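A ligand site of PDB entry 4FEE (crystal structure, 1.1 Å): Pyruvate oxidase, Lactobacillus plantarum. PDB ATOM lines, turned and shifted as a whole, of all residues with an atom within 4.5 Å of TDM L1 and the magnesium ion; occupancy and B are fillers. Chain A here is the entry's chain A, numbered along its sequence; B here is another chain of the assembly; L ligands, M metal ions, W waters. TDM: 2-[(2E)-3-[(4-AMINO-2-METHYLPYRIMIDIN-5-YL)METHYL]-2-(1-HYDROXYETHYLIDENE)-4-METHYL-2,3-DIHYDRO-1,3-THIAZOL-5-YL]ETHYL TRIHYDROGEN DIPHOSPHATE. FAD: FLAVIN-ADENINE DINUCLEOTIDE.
The side-chain carboxylate of Glu 59 of chain B sits at hydrogen-bond distance from a nitrogen (N1') of TDM L1, 2.6 Å away.
O3B of TDM L1 sits at hydrogen-bond distance from N of Phe 479 (2.9 Å).
The backbone NH (N) of Gly 448 lies within hydrogen-bond range of an oxygen (O2A) of TDM L1.
The backbone NH (N) of Met 422 is in hydrogen-bond range of a nitrogen (N3') of TDM L1 (3.3 Å).
An oxygen (O28) of TDM L1 sits at hydrogen-bond distance from the side-chain amide nitrogen (NE2) of Gln 122 of chain B (2.7 Å).
N of Gly 478 is in hydrogen-bond range of O3B of TDM L1, at 3.4 Å.
A nitrogen (N4') of TDM L1 lies within hydrogen-bond range of the backbone carbonyl oxygen of Ala 420 (2.7 Å).
The backbone NH of Asp 396 sits at hydrogen-bond distance from an oxygen (O3B) of TDM L1, at 2.9 Å.
N of Gly 449 is in hydrogen-bond range of O2A of TDM L1, 2.8 Å away.
The backbone carbonyl oxygen (O) of Phe 472 is in hydrogen-bond range of the backbone NH (N) of Asp 447.
The side-chain amide oxygen (OE1) of Gln 122 of chain B sits close to the backbone carbonyl oxygen (O) of Ala 420 (3.4 Å).
A ring nitrogen (ND1) of His 89 of chain B lies within hydrogen-bond range of the side-chain carboxylate (OE1) of Glu 59 of chain B (2.8 Å).
The side-chain amide nitrogen of Asn 92 sits close to a ring nitrogen (NE2) of His 89 of chain B (3.4 Å).
ND2 of Asn 92 is in hydrogen-bond range of O of Pro 85 of chain B.
Val 394 touches TDM L1 (O to C7, 3.5 Å).
Gly 395 touches TDM L1 (C to O3B, 3.9 Å).
CA of Gly 446 touches O2A of TDM L1, at 3.6 Å.
Met 452 touches TDM L1 (SD to CM2, 3.7 Å).
CD1 of Tyr 477 touches O7 of TDM L1 (3.4 Å).
Ile 480 touches TDM L1 (CG1 to C4, 3.4 Å).
Ile 32 of chain B touches TDM L1.
Pro 33 of chain B touches TDM L1.
OG of Ser 82 of chain B touches C6' of TDM L1, 3.1 Å away.
Pro 85 of chain B touches TDM L1 (CG to N3', 3.5 Å).
Gly 86 of chain B touches TDM L1.
His 89 of chain B touches TDM L1.
Of the 29 residues printed, 24 come within 4 Å of TDM L1.
Three residues have an atom within 4 Å of the magnesium ion: Asp 447, Asn 474 and Gln 476.
The nearest printed residue that does not touch the magnesium ion is Gly 448 (4.1 Å).
An oxygen (O1A) of TDM L1 binds the magnesium ion (2.0 Å).
The magnesium ion is bound by OD1 of Asp 447 (2.0 Å).
O of Gln 476 binds the magnesium ion (2.1 Å).
The magnesium ion is bound by water W3, 2.1 Å away.
The magnesium ion is bound by O2B of TDM L1 (2.1 Å).
OD1 of Asn 474 is bound to the magnesium ion.
Water W3 lies within hydrogen-bond range of the backbone carbonyl oxygen (O) of Phe 472 (2.6 Å), an oxygen (O1B) of TDM L1 (2.7 Å), the backbone NH (N) of Asp 447 (3.2 Å) and the side-chain amide nitrogen (ND2) of Asn 474 (3.4 Å).
Water W2 lies within hydrogen-bond range of an oxygen (O2A) of TDM L1 (2.6 Å), the backbone carbonyl oxygen of Val 394 (2.8 Å) and the backbone NH of Gly 446 (2.9 Å).
Water W5 lies within hydrogen-bond range of an oxygen (O1B) of TDM L1, the backbone NH of Ile 397 and the backbone NH of Asp 396.
Water W1 bridges OG of Ser 82 of chain B (2.7 Å) and OE1 of Gln 122 of chain B (3.2 Å).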
ATOM      1  N   ASN A  92      24.997 -11.633 -27.960  1.00  0.00           N
ATOM      2  CA  ASN A  92      24.929 -13.080 -28.056  1.00  0.00           C
ATOM      3  C   ASN A  92      24.325 -13.512 -29.388  1.00  0.00           C
ATOM      4  O   ASN A  92      24.674 -14.552 -29.917  1.00  0.00           O
ATOM      5  CB  ASN A  92      24.202 -13.726 -26.877  1.00  0.00           C
ATOM      6  CG  ASN A  92      25.153 -13.853 -25.713  1.00  0.00           C
ATOM      7  OD1 ASN A  92      25.824 -12.889 -25.346  1.00  0.00           O
ATOM      8  ND2 ASN A  92      25.209 -15.035 -25.102  1.00  0.00           N
ATOM      9  N   VAL A 394      19.939 -24.881 -25.923  1.00  0.00           N
ATOM     10  CA  VAL A 394      21.291 -25.440 -25.774  1.00  0.00           C
ATOM     11  C   VAL A 394      21.393 -26.151 -24.446  1.00  0.00           C
ATOM     12  O   VAL A 394      21.120 -25.535 -23.395  1.00  0.00           O
ATOM     13  CB  VAL A 394      22.316 -24.293 -25.887  1.00  0.00           C
ATOM     14  CG1 VAL A 394      23.716 -24.757 -25.477  1.00  0.00           C
ATOM     15  CG2 VAL A 394      22.327 -23.776 -27.287  1.00  0.00           C
ATOM     16  N   GLY A 395      21.843 -27.403 -24.466  1.00  0.00           N
ATOM     17  CA  GLY A 395      21.985 -28.198 -23.284  1.00  0.00           C
ATOM     18  C   GLY A 395      21.633 -29.653 -23.586  1.00  0.00           C
ATOM     19  O   GLY A 395      21.766 -30.118 -24.723  1.00  0.00           O
ATOM     20  N   ASP A 396      21.175 -30.386 -22.564  1.00  0.00           N
ATOM     21  CA  ASP A 396      20.756 -31.748 -22.819  1.00  0.00           C
ATOM     22  C   ASP A 396      19.727 -31.860 -23.932  1.00  0.00           C
ATOM     23  O   ASP A 396      19.651 -32.893 -24.588  1.00  0.00           O
ATOM     24  CB  ASP A 396      20.202 -32.395 -21.549  1.00  0.00           C
ATOM     25  CG  ASP A 396      21.170 -32.931 -20.567  1.00  0.00           C
ATOM     26  OD1 ASP A 396      22.355 -33.056 -20.858  1.00  0.00           O
ATOM     27  OD2 ASP A 396      20.666 -33.265 -19.425  1.00  0.00           O
ATOM     28  N   ILE A 397      18.920 -30.834 -24.184  1.00  0.00           N
ATOM     29  CA  ILE A 397      17.937 -30.920 -25.233  1.00  0.00           C
ATOM     30  C   ILE A 397      18.589 -31.183 -26.571  1.00  0.00           C
ATOM     31  O   ILE A 397      17.976 -31.866 -27.406  1.00  0.00           O
ATOM     32  CB  ILE A 397      17.023 -29.674 -25.309  1.00  0.00           C
ATOM     33  CG1 ILE A 397      15.830 -29.875 -26.249  1.00  0.00           C
ATOM     34  CG2 ILE A 397      17.781 -28.391 -25.660  1.00  0.00           C
ATOM     35  CD1 ILE A 397      14.953 -31.084 -25.948  1.00  0.00           C
ATOM     36  N   ALA A 420      26.864 -21.739 -29.510  1.00  0.00           N
ATOM     37  CA  ALA A 420      26.066 -22.445 -28.543  1.00  0.00           C
ATOM     38  C   ALA A 420      25.589 -21.528 -27.432  1.00  0.00           C
ATOM     39  O   ALA A 420      25.657 -21.872 -26.248  1.00  0.00           O
ATOM     40  CB  ALA A 420      26.786 -23.668 -28.013  1.00  0.00           C
ATOM     41  N   THR A 421      25.013 -20.390 -27.801  1.00  0.00           N
ATOM     42  CA  THR A 421      24.349 -19.552 -26.795  1.00  0.00           C
ATOM     43  C   THR A 421      23.016 -20.146 -26.343  1.00  0.00           C
ATOM     44  O   THR A 421      22.127 -20.375 -27.134  1.00  0.00           O
ATOM     45  CB  THR A 421      24.217 -18.108 -27.229  1.00  0.00           C
ATOM     46  OG1 THR A 421      23.673 -17.322 -26.156  1.00  0.00           O
ATOM     47  CG2 THR A 421      23.345 -17.923 -28.503  1.00  0.00           C
ATOM     48  N   MET A 422      22.902 -20.340 -25.018  1.00  0.00           N
ATOM     49  CA  MET A 422      21.603 -20.602 -24.449  1.00  0.00           C
ATOM     50  C   MET A 422      20.669 -19.430 -24.714  1.00  0.00           C
ATOM     51  O   MET A 422      21.109 -18.279 -24.927  1.00  0.00           O
ATOM     52  CB  MET A 422      21.778 -20.797 -22.939  1.00  0.00           C
ATOM     53  CG  MET A 422      22.494 -22.077 -22.530  1.00  0.00           C
ATOM     54  SD  MET A 422      22.967 -22.048 -20.822  1.00  0.00           S
ATOM     55  CE  MET A 422      21.385 -22.057 -20.008  1.00  0.00           C
ATOM     56  N   GLY A 446      15.619 -26.380 -22.440  1.00  0.00           N
ATOM     57  CA  GLY A 446      15.818 -26.632 -21.042  1.00  0.00           C
ATOM     58  C   GLY A 446      15.379 -25.451 -20.189  1.00  0.00           C
ATOM     59  O   GLY A 446      15.231 -24.321 -20.664  1.00  0.00           O
ATOM     60  N   ASP A 447      15.252 -25.713 -18.891  1.00  0.00           N
ATOM     61  CA  ASP A 447      14.838 -24.660 -17.961  1.00  0.00           C
ATOM     62  C   ASP A 447      15.885 -23.556 -17.845  1.00  0.00           C
ATOM     63  O   ASP A 447      15.504 -22.384 -17.742  1.00  0.00           O
ATOM     64  CB  ASP A 447      14.426 -25.235 -16.610  1.00  0.00           C
ATOM     65  CG  ASP A 447      15.335 -26.178 -15.899  1.00  0.00           C
ATOM     66  OD1 ASP A 447      16.438 -26.557 -16.443  1.00  0.00           O
ATOM     67  OD2 ASP A 447      14.987 -26.563 -14.761  1.00  0.00           O
ATOM     68  N   GLY A 448      17.171 -23.885 -17.882  1.00  0.00           N
ATOM     69  CA  GLY A 448      18.178 -22.849 -17.826  1.00  0.00           C
ATOM     70  C   GLY A 448      18.109 -21.912 -18.996  1.00  0.00           C
ATOM     71  O   GLY A 448      18.164 -20.691 -18.847  1.00  0.00           O
ATOM     72  N   GLY A 449      18.005 -22.483 -20.190  1.00  0.00           N
ATOM     73  CA  GLY A 449      17.973 -21.660 -21.413  1.00  0.00           C
ATOM     74  C   GLY A 449      16.675 -20.892 -21.565  1.00  0.00           C
ATOM     75  O   GLY A 449      16.692 -19.712 -21.931  1.00  0.00           O
ATOM     76  N   MET A 452      16.656 -17.765 -19.561  1.00  0.00           N
ATOM     77  CA  MET A 452      17.432 -16.615 -20.019  1.00  0.00           C
ATOM     78  C   MET A 452      16.658 -15.712 -20.936  1.00  0.00           C
ATOM     79  O   MET A 452      16.976 -14.518 -20.961  1.00  0.00           O
ATOM     80  CB  MET A 452      18.715 -17.102 -20.700  1.00  0.00           C
ATOM     81  CG  MET A 452      19.729 -17.558 -19.663  1.00  0.00           C
ATOM     82  SD  MET A 452      21.234 -18.106 -20.484  1.00  0.00           S
ATOM     83  CE  MET A 452      22.190 -18.556 -19.060  1.00  0.00           C
ATOM     84  N   PHE A 472      11.927 -28.228 -20.525  1.00  0.00           N
ATOM     85  CA  PHE A 472      12.384 -29.447 -19.838  1.00  0.00           C
ATOM     86  C   PHE A 472      12.960 -29.046 -18.489  1.00  0.00           C
ATOM     87  O   PHE A 472      14.091 -28.591 -18.379  1.00  0.00           O
ATOM     88  CB  PHE A 472      13.409 -30.177 -20.720  1.00  0.00           C
ATOM     89  CG  PHE A 472      12.858 -30.749 -21.996  1.00  0.00           C
ATOM     90  CD1 PHE A 472      12.420 -29.962 -23.072  1.00  0.00           C
ATOM     91  CD2 PHE A 472      12.736 -32.120 -22.125  1.00  0.00           C
ATOM     92  CE1 PHE A 472      11.874 -30.499 -24.169  1.00  0.00           C
ATOM     93  CE2 PHE A 472      12.229 -32.707 -23.297  1.00  0.00           C
ATOM     94  CZ  PHE A 472      11.751 -31.891 -24.316  1.00  0.00           C
ATOM     95  N   ASN A 474      14.394 -29.749 -15.192  1.00  0.00           N
ATOM     96  CA  ASN A 474      15.118 -30.628 -14.312  1.00  0.00           C
ATOM     97  C   ASN A 474      15.679 -29.905 -13.076  1.00  0.00           C
ATOM     98  O   ASN A 474      16.302 -30.564 -12.245  1.00  0.00           O
ATOM     99  CB  ASN A 474      16.225 -31.401 -15.058  1.00  0.00           C
ATOM    100  CG  ASN A 474      17.135 -30.558 -15.864  1.00  0.00           C
ATOM    101  OD1 ASN A 474      17.191 -29.326 -15.705  1.00  0.00           O
ATOM    102  ND2 ASN A 474      17.938 -31.186 -16.722  1.00  0.00           N
ATOM    103  N   GLN A 476      18.216 -28.081 -13.026  1.00  0.00           N
ATOM    104  CA  GLN A 476      19.639 -28.226 -13.175  1.00  0.00           C
ATOM    105  C   GLN A 476      20.123 -27.582 -14.447  1.00  0.00           C
ATOM    106  O   GLN A 476      19.348 -27.455 -15.445  1.00  0.00           O
ATOM    107  CB  GLN A 476      20.042 -29.686 -13.273  1.00  0.00           C
ATOM    108  CG  GLN A 476      19.659 -30.562 -12.126  1.00  0.00           C
ATOM    109  CD  GLN A 476      19.978 -32.022 -12.419  1.00  0.00           C
ATOM    110  OE1 GLN A 476      20.099 -32.428 -13.561  1.00  0.00           O
ATOM    111  NE2 GLN A 476      20.082 -32.811 -11.409  1.00  0.00           N
ATOM    112  N   TYR A 477      21.393 -27.249 -14.498  1.00  0.00           N
ATOM    113  CA  TYR A 477      22.142 -27.137 -15.752  1.00  0.00           C
ATOM    114  C   TYR A 477      22.660 -28.548 -16.007  1.00  0.00           C
ATOM    115  O   TYR A 477      23.821 -28.854 -15.663  1.00  0.00           O
ATOM    116  CB  TYR A 477      23.269 -26.121 -15.656  1.00  0.00           C
ATOM    117  CG  TYR A 477      22.806 -24.680 -15.431  1.00  0.00           C
ATOM    118  CD1 TYR A 477      21.902 -24.034 -16.249  1.00  0.00           C
ATOM    119  CD2 TYR A 477      23.300 -23.951 -14.376  1.00  0.00           C
ATOM    120  CE1 TYR A 477      21.518 -22.746 -16.021  1.00  0.00           C
ATOM    121  CE2 TYR A 477      22.899 -22.669 -14.139  1.00  0.00           C
ATOM    122  CZ  TYR A 477      22.004 -22.040 -14.926  1.00  0.00           C
ATOM    123  OH  TYR A 477      21.616 -20.753 -14.685  1.00  0.00           O
ATOM    124  N   GLY A 478      21.809 -29.418 -16.510  1.00  0.00           N
ATOM    125  CA  GLY A 478      22.151 -30.847 -16.543  1.00  0.00           C
ATOM    126  C   GLY A 478      23.370 -31.167 -17.356  1.00  0.00           C
ATOM    127  O   GLY A 478      24.241 -31.936 -16.933  1.00  0.00           O
ATOM    128  N   PHE A 479      23.495 -30.501 -18.511  1.00  0.00           N
ATOM    129  CA  PHE A 479      24.635 -30.754 -19.367  1.00  0.00           C
ATOM    130  C   PHE A 479      25.930 -30.445 -18.643  1.00  0.00           C
ATOM    131  O   PHE A 479      26.926 -31.145 -18.846  1.00  0.00           O
ATOM    132  CB  PHE A 479      24.482 -29.880 -20.635  1.00  0.00           C
ATOM    133  CG  PHE A 479      25.229 -30.288 -21.880  1.00  0.00           C
ATOM    134  CD1 PHE A 479      24.768 -31.363 -22.660  1.00  0.00           C
ATOM    135  CD2 PHE A 479      26.326 -29.576 -22.326  1.00  0.00           C
ATOM    136  CE1 PHE A 479      25.402 -31.726 -23.842  1.00  0.00           C
ATOM    137  CE2 PHE A 479      26.948 -29.932 -23.504  1.00  0.00           C
ATOM    138  CZ  PHE A 479      26.467 -30.993 -24.267  1.00  0.00           C
ATOM    139  N   ILE A 480      25.941 -29.402 -17.829  1.00  0.00           N
ATOM    140  CA  ILE A 480      27.134 -29.012 -17.063  1.00  0.00           C
ATOM    141  C   ILE A 480      27.324 -29.842 -15.808  1.00  0.00           C
ATOM    142  O   ILE A 480      28.455 -30.148 -15.429  1.00  0.00           O
ATOM    143  CB  ILE A 480      27.093 -27.537 -16.716  1.00  0.00           C
ATOM    144  CG1 ILE A 480      26.812 -26.708 -17.965  1.00  0.00           C
ATOM    145  CG2 ILE A 480      28.345 -27.053 -16.002  1.00  0.00           C
ATOM    146  CD1 ILE A 480      27.740 -27.008 -19.097  1.00  0.00           C
ATOM    147  N   ILE B  32      27.644 -18.330 -13.813  1.00  0.00           N
ATOM    148  CA  ILE B  32      26.978 -19.558 -14.239  1.00  0.00           C
ATOM    149  C   ILE B  32      28.081 -20.478 -14.738  1.00  0.00           C
ATOM    150  O   ILE B  32      28.961 -20.048 -15.495  1.00  0.00           O
ATOM    151  CB  ILE B  32      25.955 -19.298 -15.361  1.00  0.00           C
ATOM    152  CG1 ILE B  32      24.772 -18.479 -14.811  1.00  0.00           C
ATOM    153  CG2 ILE B  32      25.491 -20.574 -16.052  1.00  0.00           C
ATOM    154  CD1 ILE B  32      23.747 -18.060 -15.848  1.00  0.00           C
ATOM    155  N   PRO B  33      28.105 -21.738 -14.298  1.00  0.00           N
ATOM    156  CA  PRO B  33      29.213 -22.644 -14.658  1.00  0.00           C
ATOM    157  C   PRO B  33      29.107 -23.102 -16.112  1.00  0.00           C
ATOM    158  O   PRO B  33      28.081 -22.986 -16.769  1.00  0.00           O
ATOM    159  CB  PRO B  33      29.050 -23.814 -13.702  1.00  0.00           C
ATOM    160  CG  PRO B  33      27.564 -23.861 -13.506  1.00  0.00           C
ATOM    161  CD  PRO B  33      27.145 -22.407 -13.422  1.00  0.00           C
ATOM    162  N   GLU B  59      23.997 -14.346 -16.986  1.00  0.00           N
ATOM    163  CA  GLU B  59      25.263 -13.765 -16.580  1.00  0.00           C
ATOM    164  C   GLU B  59      25.286 -12.239 -16.567  1.00  0.00           C
ATOM    165  O   GLU B  59      26.091 -11.648 -15.832  1.00  0.00           O
ATOM    166  CB  GLU B  59      26.408 -14.272 -17.463  1.00  0.00           C
ATOM    167  CG  GLU B  59      26.638 -15.761 -17.482  1.00  0.00           C
ATOM    168  CD  GLU B  59      25.809 -16.524 -18.508  1.00  0.00           C
ATOM    169  OE1 GLU B  59      24.825 -15.999 -19.074  1.00  0.00           O
ATOM    170  OE2 GLU B  59      26.149 -17.732 -18.697  1.00  0.00           O
ATOM    171  N   SER B  82      31.192 -18.352 -18.673  1.00  0.00           N
ATOM    172  CA  SER B  82      31.795 -19.400 -19.476  1.00  0.00           C
ATOM    173  C   SER B  82      32.226 -18.893 -20.835  1.00  0.00           C
ATOM    174  O   SER B  82      31.899 -17.805 -21.303  1.00  0.00           O
ATOM    175  CB  SER B  82      30.806 -20.579 -19.549  1.00  0.00           C
ATOM    176  OG  SER B  82      29.592 -20.201 -20.190  1.00  0.00           O
ATOM    177  N   PRO B  85      29.427 -17.498 -25.123  1.00  0.00           N
ATOM    178  CA  PRO B  85      28.194 -16.805 -24.718  1.00  0.00           C
ATOM    179  C   PRO B  85      28.083 -16.487 -23.236  1.00  0.00           C
ATOM    180  O   PRO B  85      27.305 -15.559 -22.900  1.00  0.00           O
ATOM    181  CB  PRO B  85      27.093 -17.742 -25.158  1.00  0.00           C
ATOM    182  CG  PRO B  85      27.751 -19.111 -25.193  1.00  0.00           C
ATOM    183  CD  PRO B  85      29.116 -18.783 -25.747  1.00  0.00           C
ATOM    184  N   GLY B  86      28.721 -17.194 -22.337  1.00  0.00           N
ATOM    185  CA  GLY B  86      28.646 -16.810 -20.926  1.00  0.00           C
ATOM    186  C   GLY B  86      29.292 -15.454 -20.690  1.00  0.00           C
ATOM    187  O   GLY B  86      28.703 -14.573 -20.097  1.00  0.00           O
ATOM    188  N   HIS B  89      27.499 -12.418 -22.411  1.00  0.00           N
ATOM    189  CA  HIS B  89      26.367 -11.982 -21.600  1.00  0.00           C
ATOM    190  C   HIS B  89      26.734 -11.010 -20.487  1.00  0.00           C
ATOM    191  O   HIS B  89      25.851 -10.320 -19.989  1.00  0.00           O
ATOM    192  CB  HIS B  89      25.633 -13.168 -21.011  1.00  0.00           C
ATOM    193  CG  HIS B  89      24.465 -13.698 -21.776  1.00  0.00           C
ATOM    194  ND1 HIS B  89      23.804 -14.829 -21.382  1.00  0.00           N
ATOM    195  CD2 HIS B  89      23.767 -13.194 -22.825  1.00  0.00           C
ATOM    196  CE1 HIS B  89      22.763 -15.017 -22.169  1.00  0.00           C
ATOM    197  NE2 HIS B  89      22.733 -14.031 -23.079  1.00  0.00           N
ATOM    198  N   PHE B 121      34.692 -26.530 -30.437  1.00  0.00           N
ATOM    199  CA  PHE B 121      33.394 -26.125 -29.989  1.00  0.00           C
ATOM    200  C   PHE B 121      33.479 -24.927 -29.056  1.00  0.00           C
ATOM    201  O   PHE B 121      34.208 -24.975 -28.073  1.00  0.00           O
ATOM    202  CB  PHE B 121      32.760 -27.307 -29.290  1.00  0.00           C
ATOM    203  CG  PHE B 121      31.354 -27.013 -28.733  1.00  0.00           C
ATOM    204  CD1 PHE B 121      30.278 -26.896 -29.567  1.00  0.00           C
ATOM    205  CD2 PHE B 121      31.176 -26.826 -27.388  1.00  0.00           C
ATOM    206  CE1 PHE B 121      29.026 -26.612 -29.086  1.00  0.00           C
ATOM    207  CE2 PHE B 121      29.899 -26.583 -26.868  1.00  0.00           C
ATOM    208  CZ  PHE B 121      28.828 -26.464 -27.737  1.00  0.00           C
ATOM    209  N   GLN B 122      32.727 -23.848 -29.229  1.00  0.00           N
ATOM    210  CA  GLN B 122      32.662 -22.662 -28.395  1.00  0.00           C
ATOM    211  C   GLN B 122      34.025 -22.007 -28.264  1.00  0.00           C
ATOM    212  O   GLN B 122      34.281 -21.195 -27.374  1.00  0.00           O
ATOM    213  CB  GLN B 122      32.049 -22.873 -27.006  1.00  0.00           C
ATOM    214  CG  GLN B 122      30.575 -23.227 -27.172  1.00  0.00           C
ATOM    215  CD  GLN B 122      29.801 -23.147 -25.906  1.00  0.00           C
ATOM    216  OE1 GLN B 122      28.994 -22.251 -25.629  1.00  0.00           O
ATOM    217  NE2 GLN B 122      30.048 -24.121 -25.092  1.00  0.00           N
HETATM  218  O1A TDM L   1      18.727 -26.222 -18.012  1.00  0.00           O
HETATM  219  PA  TDM L   1      19.494 -26.146 -19.302  1.00  0.00           P
HETATM  220  O2A TDM L   1      18.989 -25.149 -20.317  1.00  0.00           O
HETATM  221  O3A TDM L   1      19.511 -27.560 -20.012  1.00  0.00           O
HETATM  222  PB  TDM L   1      19.694 -29.068 -19.401  1.00  0.00           P
HETATM  223  O2B TDM L   1      19.475 -28.958 -17.905  1.00  0.00           O
HETATM  224  O3B TDM L   1      21.041 -29.551 -19.781  1.00  0.00           O
HETATM  225  O1B TDM L   1      18.556 -29.809 -20.089  1.00  0.00           O
HETATM  226  O7  TDM L   1      21.007 -25.870 -18.919  1.00  0.00           O
HETATM  227  C7  TDM L   1      22.014 -25.622 -19.999  1.00  0.00           C
HETATM  228  C6  TDM L   1      23.368 -25.759 -19.304  1.00  0.00           C
HETATM  229  C5  TDM L   1      24.517 -25.289 -20.174  1.00  0.00           C
HETATM  230  S1  TDM L   1      24.868 -26.095 -21.656  1.00  0.00           S
HETATM  231  C2  TDM L   1      26.094 -24.891 -22.107  1.00  0.00           C
HETATM  232  C27 TDM L   1      27.232 -25.411 -22.918  1.00  0.00           C
HETATM  233  C29 TDM L   1      26.743 -26.319 -24.044  1.00  0.00           C
HETATM  234  O28 TDM L   1      27.943 -24.349 -23.498  1.00  0.00           O
HETATM  235  N3  TDM L   1      26.323 -24.085 -20.918  1.00  0.00           N
HETATM  236  C4  TDM L   1      25.347 -24.269 -19.895  1.00  0.00           C
HETATM  237  CM4 TDM L   1      25.391 -23.411 -18.668  1.00  0.00           C
HETATM  238  C7' TDM L   1      27.218 -22.951 -20.950  1.00  0.00           C
HETATM  239  C5' TDM L   1      26.559 -21.619 -21.327  1.00  0.00           C
HETATM  240  C4' TDM L   1      26.045 -21.349 -22.593  1.00  0.00           C
HETATM  241  N4' TDM L   1      26.217 -22.181 -23.576  1.00  0.00           N
HETATM  242  N3' TDM L   1      25.376 -20.147 -22.866  1.00  0.00           N
HETATM  243  C2' TDM L   1      25.299 -19.228 -21.818  1.00  0.00           C
HETATM  244  CM2 TDM L   1      24.578 -17.981 -22.142  1.00  0.00           C
HETATM  245  N1' TDM L   1      25.851 -19.421 -20.658  1.00  0.00           N
HETATM  246  C6' TDM L   1      26.531 -20.630 -20.366  1.00  0.00           C
HETATM  247  PA  FAD L   2      29.228 -26.118 -40.485  1.00  0.00           P
HETATM  248  O1A FAD L   2      28.363 -24.964 -40.765  1.00  0.00           O
HETATM  249  O2A FAD L   2      30.259 -25.984 -39.398  1.00  0.00           O
HETATM  250  O5B FAD L   2      30.024 -26.552 -41.769  1.00  0.00           O
HETATM  251  C5B FAD L   2      29.352 -26.690 -43.054  1.00  0.00           C
HETATM  252  C4B FAD L   2      30.469 -27.027 -44.040  1.00  0.00           C
HETATM  253  O4B FAD L   2      29.855 -27.208 -45.332  1.00  0.00           O
HETATM  254  C3B FAD L   2      31.552 -25.914 -44.228  1.00  0.00           C
HETATM  255  O3B FAD L   2      32.875 -26.485 -44.241  1.00  0.00           O
HETATM  256  C2B FAD L   2      31.147 -25.331 -45.548  1.00  0.00           C
HETATM  257  O2B FAD L   2      32.228 -24.681 -46.263  1.00  0.00           O
HETATM  258  C1B FAD L   2      30.572 -26.457 -46.337  1.00  0.00           C
HETATM  259  N9A FAD L   2      29.713 -26.180 -47.422  1.00  0.00           N
HETATM  260  C8A FAD L   2      28.710 -25.241 -47.398  1.00  0.00           C
HETATM  261  N7A FAD L   2      27.973 -25.304 -48.547  1.00  0.00           N
HETATM  262  C5A FAD L   2      28.552 -26.318 -49.278  1.00  0.00           C
HETATM  263  C6A FAD L   2      28.216 -26.855 -50.543  1.00  0.00           C
HETATM  264  N6A FAD L   2      27.295 -26.375 -51.371  1.00  0.00           N
HETATM  265  N1A FAD L   2      28.986 -27.914 -50.964  1.00  0.00           N
HETATM  266  C2A FAD L   2      30.027 -28.364 -50.226  1.00  0.00           C
HETATM  267  N3A FAD L   2      30.397 -27.889 -49.009  1.00  0.00           N
HETATM  268  C4A FAD L   2      29.599 -26.872 -48.580  1.00  0.00           C
HETATM  269  N1  FAD L   2      27.830 -31.609 -33.363  1.00  0.00           N
HETATM  270  C2  FAD L   2      28.156 -32.937 -33.427  1.00  0.00           C
HETATM  271  O2  FAD L   2      28.110 -33.518 -34.534  1.00  0.00           O
HETATM  272  N3  FAD L   2      28.473 -33.606 -32.275  1.00  0.00           N
HETATM  273  C4  FAD L   2      28.467 -33.052 -31.032  1.00  0.00           C
HETATM  274  O4  FAD L   2      28.767 -33.728 -30.014  1.00  0.00           O
HETATM  275  C4X FAD L   2      28.008 -31.686 -30.949  1.00  0.00           C
HETATM  276  N5  FAD L   2      28.018 -31.041 -29.727  1.00  0.00           N
HETATM  277  C5X FAD L   2      27.180 -29.936 -29.626  1.00  0.00           C
HETATM  278  C6  FAD L   2      26.726 -29.509 -28.389  1.00  0.00           C
HETATM  279  C7  FAD L   2      25.834 -28.423 -28.294  1.00  0.00           C
HETATM  280  C7M FAD L   2      25.361 -27.969 -26.932  1.00  0.00           C
HETATM  281  C8  FAD L   2      25.451 -27.767 -29.471  1.00  0.00           C
HETATM  282  C8M FAD L   2      24.485 -26.602 -29.424  1.00  0.00           C
HETATM  283  C9  FAD L   2      25.923 -28.188 -30.717  1.00  0.00           C
HETATM  284  C9A FAD L   2      26.803 -29.267 -30.807  1.00  0.00           C
HETATM  285  N10 FAD L   2      27.322 -29.714 -32.047  1.00  0.00           N
HETATM  286  C10 FAD L   2      27.731 -31.034 -32.127  1.00  0.00           C
HETATM  287  C1' FAD L   2      27.359 -28.888 -33.245  1.00  0.00           C
HETATM  288  C2' FAD L   2      28.821 -28.522 -33.571  1.00  0.00           C
HETATM  289  O2' FAD L   2      29.287 -27.518 -32.638  1.00  0.00           O
HETATM  290  C3' FAD L   2      29.050 -28.055 -34.991  1.00  0.00           C
HETATM  291  O3' FAD L   2      28.233 -26.894 -35.239  1.00  0.00           O
HETATM  292  C4' FAD L   2      28.663 -29.086 -36.042  1.00  0.00           C
HETATM  293  O4' FAD L   2      29.215 -30.404 -35.710  1.00  0.00           O
HETATM  294  C5' FAD L   2      29.215 -28.706 -37.388  1.00  0.00           C
HETATM  295  O5' FAD L   2      28.232 -29.119 -38.384  1.00  0.00           O
HETATM  296  P   FAD L   2      28.457 -28.910 -39.924  1.00  0.00           P
HETATM  297  O1P FAD L   2      29.832 -29.308 -40.329  1.00  0.00           O
HETATM  298  O2P FAD L   2      27.276 -29.591 -40.537  1.00  0.00           O
HETATM  299  O3P FAD L   2      28.250 -27.342 -40.160  1.00  0.00           O
HETATM  300 MG    MG M   1      17.987 -27.797 -16.950  1.00  0.00          MG
HETATM  301  O   HOH W   1      29.768 -21.388 -22.614  1.00  0.00           O
HETATM  302  O   HOH W   2      18.373 -25.674 -22.839  1.00  0.00           O
HETATM  303  O   HOH W   3      16.736 -28.514 -18.495  1.00  0.00           O
HETATM  304  O   HOH W   4      29.563 -27.750 -22.369  1.00  0.00           O
HETATM  305  O   HOH W   5      18.322 -28.607 -22.554  1.00  0.00           O
HETATM  306  O   HOH W   6      16.765 -31.869 -20.355  1.00  0.00           O
